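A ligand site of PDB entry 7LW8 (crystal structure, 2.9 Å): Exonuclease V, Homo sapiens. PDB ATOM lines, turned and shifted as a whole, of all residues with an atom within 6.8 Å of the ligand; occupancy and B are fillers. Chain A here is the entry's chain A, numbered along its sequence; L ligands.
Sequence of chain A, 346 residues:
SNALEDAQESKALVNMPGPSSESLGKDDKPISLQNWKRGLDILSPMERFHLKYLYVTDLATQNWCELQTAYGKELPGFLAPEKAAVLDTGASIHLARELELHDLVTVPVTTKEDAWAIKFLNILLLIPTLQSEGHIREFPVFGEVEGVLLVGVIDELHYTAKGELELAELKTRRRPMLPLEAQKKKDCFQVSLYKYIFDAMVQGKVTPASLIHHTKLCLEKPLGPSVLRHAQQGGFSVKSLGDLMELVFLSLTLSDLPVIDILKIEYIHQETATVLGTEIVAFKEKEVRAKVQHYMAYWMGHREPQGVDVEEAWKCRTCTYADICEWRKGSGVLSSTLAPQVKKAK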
ATOM      1  N   TRP A  64       7.138 -22.560   9.562  1.00  0.00           N
ATOM      2  CA  TRP A  64       8.382 -23.320   9.624  1.00  0.00           C
ATOM      3  C   TRP A  64       9.404 -22.617  10.517  1.00  0.00           C
ATOM      4  O   TRP A  64       9.844 -23.172  11.538  1.00  0.00           O
ATOM      5  CB  TRP A  64       8.935 -23.518   8.211  1.00  0.00           C
ATOM      6  CG  TRP A  64      10.174 -24.351   8.154  1.00  0.00           C
ATOM      7  CD1 TRP A  64      11.464 -23.894   8.085  1.00  0.00           C
ATOM      8  CD2 TRP A  64      10.257 -25.785   8.142  1.00  0.00           C
ATOM      9  NE1 TRP A  64      12.336 -24.957   8.046  1.00  0.00           N
ATOM     10  CE2 TRP A  64      11.617 -26.121   8.079  1.00  0.00           C
ATOM     11  CE3 TRP A  64       9.303 -26.803   8.183  1.00  0.00           C
ATOM     12  CZ2 TRP A  64      12.062 -27.444   8.052  1.00  0.00           C
ATOM     13  CZ3 TRP A  64       9.745 -28.121   8.164  1.00  0.00           C
ATOM     14  CH2 TRP A  64      11.108 -28.433   8.098  1.00  0.00           C
ATOM     15  N   CYS A  65       9.780 -21.393  10.160  1.00  0.00           N
ATOM     16  CA  CYS A  65      10.612 -20.547  11.005  1.00  0.00           C
ATOM     17  C   CYS A  65      10.358 -19.096  10.614  1.00  0.00           C
ATOM     18  O   CYS A  65      10.615 -18.709   9.473  1.00  0.00           O
ATOM     19  CB  CYS A  65      12.094 -20.883  10.851  1.00  0.00           C
ATOM     20  SG  CYS A  65      13.166 -19.780  11.799  1.00  0.00           S
ATOM     21  N   GLU A  66       9.843 -18.312  11.568  1.00  0.00           N
ATOM     22  CA  GLU A  66       9.504 -16.917  11.284  1.00  0.00           C
ATOM     23  C   GLU A  66      10.747 -16.121  10.874  1.00  0.00           C
ATOM     24  O   GLU A  66      10.677 -15.280   9.978  1.00  0.00           O
ATOM     25  CB  GLU A  66       8.830 -16.293  12.510  1.00  0.00           C
ATOM     26  CG  GLU A  66       8.520 -14.814  12.410  1.00  0.00           C
ATOM     27  CD  GLU A  66       7.659 -14.347  13.564  1.00  0.00           C
ATOM     28  OE1 GLU A  66       6.419 -14.337  13.412  1.00  0.00           O
ATOM     29  OE2 GLU A  66       8.219 -14.004  14.625  1.00  0.00           O
ATOM     30  N   LEU A  67      11.880 -16.377  11.532  1.00  0.00           N
ATOM     31  CA  LEU A  67      13.108 -15.653  11.204  1.00  0.00           C
ATOM     32  C   LEU A  67      13.623 -16.017   9.812  1.00  0.00           C
ATOM     33  O   LEU A  67      14.176 -15.156   9.110  1.00  0.00           O
ATOM     34  CB  LEU A  67      14.169 -15.931  12.257  1.00  0.00           C
ATOM     35  CG  LEU A  67      15.307 -14.918  12.424  1.00  0.00           C
ATOM     36  CD1 LEU A  67      14.812 -13.502  12.201  1.00  0.00           C
ATOM     37  CD2 LEU A  67      15.925 -15.054  13.810  1.00  0.00           C
ATOM     38  N   GLN A  68      13.450 -17.274   9.393  1.00  0.00           N
ATOM     39  CA  GLN A  68      13.860 -17.666   8.052  1.00  0.00           C
ATOM     40  C   GLN A  68      13.028 -16.975   6.993  1.00  0.00           C
ATOM     41  O   GLN A  68      13.560 -16.559   5.946  1.00  0.00           O
ATOM     42  CB  GLN A  68      13.765 -19.186   7.909  1.00  0.00           C
ATOM     43  CG  GLN A  68      14.179 -19.713   6.547  1.00  0.00           C
ATOM     44  CD  GLN A  68      14.008 -21.225   6.431  1.00  0.00           C
ATOM     45  OE1 GLN A  68      14.746 -21.995   7.044  1.00  0.00           O
ATOM     46  NE2 GLN A  68      13.015 -21.643   5.650  1.00  0.00           N
ATOM     47  N   THR A  69      11.717 -16.839   7.225  1.00  0.00           N
ATOM     48  CA  THR A  69      10.874 -16.077   6.318  1.00  0.00           C
ATOM     49  C   THR A  69      11.318 -14.629   6.220  1.00  0.00           C
ATOM     50  O   THR A  69      11.304 -14.032   5.143  1.00  0.00           O
ATOM     51  CB  THR A  69       9.416 -16.157   6.764  1.00  0.00           C
ATOM     52  OG1 THR A  69       8.990 -17.532   6.794  1.00  0.00           O
ATOM     53  CG2 THR A  69       8.515 -15.367   5.826  1.00  0.00           C
ATOM     54  N   TYR A  71      14.427 -13.395   6.698  1.00  0.00           N
ATOM     55  CA  TYR A  71      15.648 -13.316   5.911  1.00  0.00           C
ATOM     56  C   TYR A  71      15.379 -13.539   4.429  1.00  0.00           C
ATOM     57  O   TYR A  71      16.080 -12.979   3.584  1.00  0.00           O
ATOM     58  CB  TYR A  71      16.660 -14.354   6.412  1.00  0.00           C
ATOM     59  CG  TYR A  71      17.399 -13.947   7.670  1.00  0.00           C
ATOM     60  CD1 TYR A  71      17.973 -12.687   7.793  1.00  0.00           C
ATOM     61  CD2 TYR A  71      17.530 -14.832   8.736  1.00  0.00           C
ATOM     62  CE1 TYR A  71      18.654 -12.318   8.937  1.00  0.00           C
ATOM     63  CE2 TYR A  71      18.211 -14.474   9.888  1.00  0.00           C
ATOM     64  CZ  TYR A  71      18.764 -13.219   9.980  1.00  0.00           C
ATOM     65  OH  TYR A  71      19.438 -12.857  11.127  1.00  0.00           O
ATOM     66  N   GLN A 306      10.973 -14.302  15.512  1.00  0.00           N
ATOM     67  CA  GLN A 306      11.409 -15.385  16.379  1.00  0.00           C
ATOM     68  C   GLN A 306      11.885 -16.565  15.551  1.00  0.00           C
ATOM     69  O   GLN A 306      11.321 -16.862  14.495  1.00  0.00           O
ATOM     70  CB  GLN A 306      10.279 -15.833  17.315  1.00  0.00           C
ATOM     71  CG  GLN A 306       9.698 -14.717  18.168  1.00  0.00           C
ATOM     72  CD  GLN A 306      10.464 -14.505  19.454  1.00  0.00           C
ATOM     73  OE1 GLN A 306      10.411 -15.341  20.360  1.00  0.00           O
ATOM     74  NE2 GLN A 306      11.172 -13.388  19.552  1.00  0.00           N
ATOM     75  N   GLY A 307      12.929 -17.237  16.033  1.00  0.00           N
ATOM     76  CA  GLY A 307      13.454 -18.422  15.382  1.00  0.00           C
ATOM     77  C   GLY A 307      12.758 -19.682  15.848  1.00  0.00           C
ATOM     78  O   GLY A 307      11.716 -19.655  16.523  1.00  0.00           O
ATOM     79  N   VAL A 308      13.351 -20.825  15.492  1.00  0.00           N
ATOM     80  CA  VAL A 308      12.777 -22.114  15.862  1.00  0.00           C
ATOM     81  C   VAL A 308      13.035 -22.395  17.337  1.00  0.00           C
ATOM     82  O   VAL A 308      13.940 -21.832  17.970  1.00  0.00           O
ATOM     83  CB  VAL A 308      13.337 -23.247  14.986  1.00  0.00           C
ATOM     84  CG1 VAL A 308      13.113 -22.953  13.516  1.00  0.00           C
ATOM     85  CG2 VAL A 308      14.812 -23.472  15.266  1.00  0.00           C
ATOM     86  N   GLU A 312      13.484 -28.025  17.609  1.00  0.00           N
ATOM     87  CA  GLU A 312      13.560 -28.040  16.154  1.00  0.00           C
ATOM     88  C   GLU A 312      14.833 -27.386  15.636  1.00  0.00           C
ATOM     89  O   GLU A 312      14.828 -26.751  14.576  1.00  0.00           O
ATOM     90  CB  GLU A 312      12.324 -27.368  15.554  1.00  0.00           C
ATOM     91  CG  GLU A 312      11.024 -28.096  15.841  1.00  0.00           C
ATOM     92  CD  GLU A 312       9.833 -27.445  15.172  1.00  0.00           C
ATOM     93  OE1 GLU A 312      10.018 -26.448  14.455  1.00  0.00           O
ATOM     94  OE2 GLU A 312       8.699 -27.933  15.378  1.00  0.00           O
ATOM     95  N   ALA A 313      15.942 -27.528  16.373  1.00  0.00           N
ATOM     96  CA  ALA A 313      17.217 -26.978  15.928  1.00  0.00           C
ATOM     97  C   ALA A 313      17.772 -27.675  14.701  1.00  0.00           C
ATOM     98  O   ALA A 313      18.719 -27.166  14.096  1.00  0.00           O
ATOM     99  CB  ALA A 313      18.247 -27.049  17.069  1.00  0.00           C
ATOM    100  N   LYS A 315      16.328 -27.776  11.944  1.00  0.00           N
ATOM    101  CA  LYS A 315      15.976 -26.968  10.788  1.00  0.00           C
ATOM    102  C   LYS A 315      17.108 -26.023  10.397  1.00  0.00           C
ATOM    103  O   LYS A 315      17.285 -25.730   9.210  1.00  0.00           O
ATOM    104  CB  LYS A 315      14.712 -26.167  11.072  1.00  0.00           C
ATOM    105  CG  LYS A 315      13.465 -27.008  11.281  1.00  0.00           C
ATOM    106  CD  LYS A 315      12.318 -26.162  11.788  1.00  0.00           C
ATOM    107  CE  LYS A 315      10.971 -26.766  11.435  1.00  0.00           C
ATOM    108  NZ  LYS A 315       9.844 -25.939  11.939  1.00  0.00           N
ATOM    109  N   CYS A 316      17.877 -25.537  11.371  1.00  0.00           N
ATOM    110  CA  CYS A 316      18.968 -24.617  11.096  1.00  0.00           C
ATOM    111  C   CYS A 316      20.118 -25.266  10.340  1.00  0.00           C
ATOM    112  O   CYS A 316      21.028 -24.550   9.899  1.00  0.00           O
ATOM    113  CB  CYS A 316      19.479 -24.004  12.400  1.00  0.00           C
ATOM    114  SG  CYS A 316      18.172 -23.390  13.485  1.00  0.00           S
ATOM    115  N   ARG A 317      20.115 -26.596  10.182  1.00  0.00           N
ATOM    116  CA  ARG A 317      21.169 -27.252   9.430  1.00  0.00           C
ATOM    117  C   ARG A 317      21.017 -26.991   7.935  1.00  0.00           C
ATOM    118  O   ARG A 317      21.994 -26.660   7.246  1.00  0.00           O
ATOM    119  CB  ARG A 317      21.165 -28.754   9.709  1.00  0.00           C
ATOM    120  CG  ARG A 317      22.299 -29.522   9.053  1.00  0.00           C
ATOM    121  CD  ARG A 317      22.219 -31.004   9.350  1.00  0.00           C
ATOM    122  NE  ARG A 317      21.096 -31.637   8.662  1.00  0.00           N
ATOM    123  CZ  ARG A 317      21.135 -32.093   7.416  1.00  0.00           C
ATOM    124  NH1 ARG A 317      20.064 -32.660   6.870  1.00  0.00           N
ATOM    125  NH2 ARG A 317      22.254 -31.992   6.712  1.00  0.00           N
ATOM    126  N   THR A 318      19.802 -27.116   7.413  1.00  0.00           N
ATOM    127  CA  THR A 318      19.523 -26.939   5.987  1.00  0.00           C
ATOM    128  C   THR A 318      18.993 -25.550   5.665  1.00  0.00           C
ATOM    129  O   THR A 318      18.295 -25.378   4.657  1.00  0.00           O
ATOM    130  CB  THR A 318      18.533 -28.013   5.514  1.00  0.00           C
ATOM    131  OG1 THR A 318      17.424 -28.062   6.416  1.00  0.00           O
ATOM    132  CG2 THR A 318      19.205 -29.366   5.473  1.00  0.00           C
ATOM    133  N   CYS A 319      19.307 -24.559   6.490  1.00  0.00           N
ATOM    134  CA  CYS A 319      18.820 -23.195   6.305  1.00  0.00           C
ATOM    135  C   CYS A 319      19.898 -22.353   5.643  1.00  0.00           C
ATOM    136  O   CYS A 319      21.047 -22.361   6.075  1.00  0.00           O
ATOM    137  CB  CYS A 319      18.415 -22.583   7.652  1.00  0.00           C
ATOM    138  SG  CYS A 319      17.746 -20.919   7.546  1.00  0.00           S
ATOM    139  N   THR A 320      19.506 -21.611   4.604  1.00  0.00           N
ATOM    140  CA  THR A 320      20.463 -20.795   3.858  1.00  0.00           C
ATOM    141  C   THR A 320      21.138 -19.776   4.762  1.00  0.00           C
ATOM    142  O   THR A 320      22.339 -19.521   4.627  1.00  0.00           O
ATOM    143  CB  THR A 320      19.759 -20.085   2.698  1.00  0.00           C
ATOM    144  OG1 THR A 320      18.962 -21.027   1.960  1.00  0.00           O
ATOM    145  CG2 THR A 320      20.764 -19.439   1.768  1.00  0.00           C
ATOM    146  N   TYR A 321      20.388 -19.177   5.680  1.00  0.00           N
ATOM    147  CA  TYR A 321      20.864 -18.070   6.506  1.00  0.00           C
ATOM    148  C   TYR A 321      21.428 -18.530   7.847  1.00  0.00           C
ATOM    149  O   TYR A 321      21.407 -17.761   8.811  1.00  0.00           O
ATOM    150  CB  TYR A 321      19.748 -17.056   6.708  1.00  0.00           C
ATOM    151  CG  TYR A 321      18.974 -16.756   5.440  1.00  0.00           C
ATOM    152  CD1 TYR A 321      17.789 -17.420   5.144  1.00  0.00           C
ATOM    153  CD2 TYR A 321      19.439 -15.810   4.528  1.00  0.00           C
ATOM    154  CE1 TYR A 321      17.091 -17.157   3.983  1.00  0.00           C
ATOM    155  CE2 TYR A 321      18.747 -15.539   3.366  1.00  0.00           C
ATOM    156  CZ  TYR A 321      17.579 -16.211   3.095  1.00  0.00           C
ATOM    157  OH  TYR A 321      16.884 -15.935   1.940  1.00  0.00           O
ATOM    158  N   ALA A 322      21.931 -19.763   7.923  1.00  0.00           N
ATOM    159  CA  ALA A 322      22.431 -20.267   9.203  1.00  0.00           C
ATOM    160  C   ALA A 322      23.701 -19.554   9.642  1.00  0.00           C
ATOM    161  O   ALA A 322      23.966 -19.453  10.848  1.00  0.00           O
ATOM    162  CB  ALA A 322      22.687 -21.772   9.106  1.00  0.00           C
ATOM    163  N   ASP A 323      24.491 -19.047   8.705  1.00  0.00           N
ATOM    164  CA  ASP A 323      25.770 -18.411   9.007  1.00  0.00           C
ATOM    165  C   ASP A 323      25.646 -16.911   9.253  1.00  0.00           C
ATOM    166  O   ASP A 323      26.680 -16.234   9.324  1.00  0.00           O
ATOM    167  CB  ASP A 323      26.775 -18.681   7.883  1.00  0.00           C
ATOM    168  CG  ASP A 323      26.154 -18.540   6.505  1.00  0.00           C
ATOM    169  OD1 ASP A 323      24.936 -18.294   6.420  1.00  0.00           O
ATOM    170  OD2 ASP A 323      26.887 -18.707   5.503  1.00  0.00           O
ATOM    171  N   CYS A 325      22.440 -15.865  11.020  1.00  0.00           N
ATOM    172  CA  CYS A 325      21.320 -15.821  11.970  1.00  0.00           C
ATOM    173  C   CYS A 325      21.857 -15.802  13.395  1.00  0.00           C
ATOM    174  O   CYS A 325      22.530 -16.747  13.832  1.00  0.00           O
ATOM    175  CB  CYS A 325      20.410 -17.028  11.748  1.00  0.00           C
ATOM    176  SG  CYS A 325      18.885 -17.028  12.713  1.00  0.00           S
ATOM    177  N   GLU A 326      21.562 -14.728  14.140  1.00  0.00           N
ATOM    178  CA  GLU A 326      22.013 -14.592  15.514  1.00  0.00           C
ATOM    179  C   GLU A 326      21.154 -15.366  16.503  1.00  0.00           C
ATOM    180  O   GLU A 326      21.571 -15.559  17.652  1.00  0.00           O
ATOM    181  CB  GLU A 326      22.063 -13.119  15.914  1.00  0.00           C
ATOM    182  CG  GLU A 326      22.946 -12.268  15.024  1.00  0.00           C
ATOM    183  CD  GLU A 326      24.327 -12.855  14.833  1.00  0.00           C
ATOM    184  OE1 GLU A 326      25.002 -13.114  15.853  1.00  0.00           O
ATOM    185  OE2 GLU A 326      24.737 -13.056  13.669  1.00  0.00           O
ATOM    186  N   TRP A 327      19.954 -15.805  16.085  1.00  0.00           N
ATOM    187  CA  TRP A 327      19.191 -16.732  16.898  1.00  0.00           C
ATOM    188  C   TRP A 327      19.913 -18.054  17.062  1.00  0.00           C
ATOM    189  O   TRP A 327      19.781 -18.723  18.102  1.00  0.00           O
ATOM    190  CB  TRP A 327      17.818 -16.957  16.263  1.00  0.00           C
ATOM    191  CG  TRP A 327      16.832 -17.700  17.114  1.00  0.00           C
ATOM    192  CD1 TRP A 327      16.745 -19.049  17.279  1.00  0.00           C
ATOM    193  CD2 TRP A 327      15.780 -17.131  17.901  1.00  0.00           C
ATOM    194  NE1 TRP A 327      15.708 -19.361  18.122  1.00  0.00           N
ATOM    195  CE2 TRP A 327      15.091 -18.198  18.520  1.00  0.00           C
ATOM    196  CE3 TRP A 327      15.346 -15.820  18.145  1.00  0.00           C
ATOM    197  CZ2 TRP A 327      14.011 -18.000  19.369  1.00  0.00           C
ATOM    198  CZ3 TRP A 327      14.269 -15.627  18.986  1.00  0.00           C
ATOM    199  CH2 TRP A 327      13.616 -16.705  19.590  1.00  0.00           C
ATOM    200  N   ARG A 328      20.699 -18.445  16.069  1.00  0.00           N
ATOM    201  CA  ARG A 328      21.424 -19.710  16.067  1.00  0.00           C
ATOM    202  C   ARG A 328      22.801 -19.561  16.692  1.00  0.00           C
ATOM    203  O   ARG A 328      22.994 -18.807  17.653  1.00  0.00           O
ATOM    204  CB  ARG A 328      21.534 -20.242  14.646  1.00  0.00           C
ATOM    205  CG  ARG A 328      21.726 -21.749  14.537  1.00  0.00           C
ATOM    206  CD  ARG A 328      23.202 -22.103  14.393  1.00  0.00           C
ATOM    207  NE  ARG A 328      23.394 -23.219  13.481  1.00  0.00           N
ATOM    208  CZ  ARG A 328      23.202 -24.494  13.808  1.00  0.00           C
ATOM    209  NH1 ARG A 328      22.792 -24.817  15.022  1.00  0.00           N
ATOM    210  NH2 ARG A 328      23.403 -25.448  12.904  1.00  0.00           N
HETATM  211 FE1  LIG L   1      17.904 -18.947  11.987  1.00  0.00          FE
HETATM  212 FE2  LIG L   1      17.439 -20.453   9.749  1.00  0.00          FE
HETATM  213 FE3  LIG L   1      15.407 -19.982  11.525  1.00  0.00          FE
HETATM  214 FE4  LIG L   1      17.473 -21.641  12.209  1.00  0.00          FE
HETATM  215  S1  LIG L   1      15.936 -21.972  10.555  1.00  0.00           S
HETATM  216  S2  LIG L   1      16.551 -20.000  13.497  1.00  0.00           S
HETATM  217  S3  LIG L   1      19.222 -20.623  11.168  1.00  0.00           S
HETATM  218  S4  LIG L   1      16.511 -18.434  10.266  1.00  0.00           S
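SG of Cys 325 sits close to N of Trp 327.
SG of Cys 319 sits close to N of Tyr 321 (3.7 Å).
OE1 of Gln 68 sits close to SG of Cys 319 (3.2 Å).
N of Leu 67 is in hydrogen-bond range of O of Gln 306.
The side-chain sulfur (SG) of Cys 65 lies close to the backbone NH (N) of Leu 67 (3.6 Å).
OG1 of Thr 69 sits at hydrogen-bond distance from O of Cys 65 (3.3 Å).
The side-chain sulfur (SG) of Cys 65 sits close to the backbone NH (N) of Gln 68, 3.5 Å away.
The backbone carbonyl oxygen (O) of Val 308 is in hydrogen-bond range of the indole nitrogen (NE1) of Trp 327 (3.0 Å).
The side-chain sulfur (SG) of Cys 325 binds an iron atom (FE1) of the ligand (2.3 Å).
The side-chain sulfur (SG) of Cys 65 binds an iron atom (FE3) of the ligand (2.3 Å).
OE1 of Gln 68 sits close to S1 of the ligand (3.7 Å).
An iron atom (FE4) of the ligand is bound by the side-chain sulfur of Cys 316 (2.3 Å).
The side-chain sulfur (SG) of Cys 319 binds an iron atom (FE2) of the ligand, at 2.3 Å.
S4 of the ligand sits close to N of Gln 68, at 3.4 Å.
Residues that only touch the ligand: Leu 67, Gly 307, Val 308, Ala 322 and Trp 327.
The nearest printed residue that does not touch the ligand is Tyr 71 (4.04 Å).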
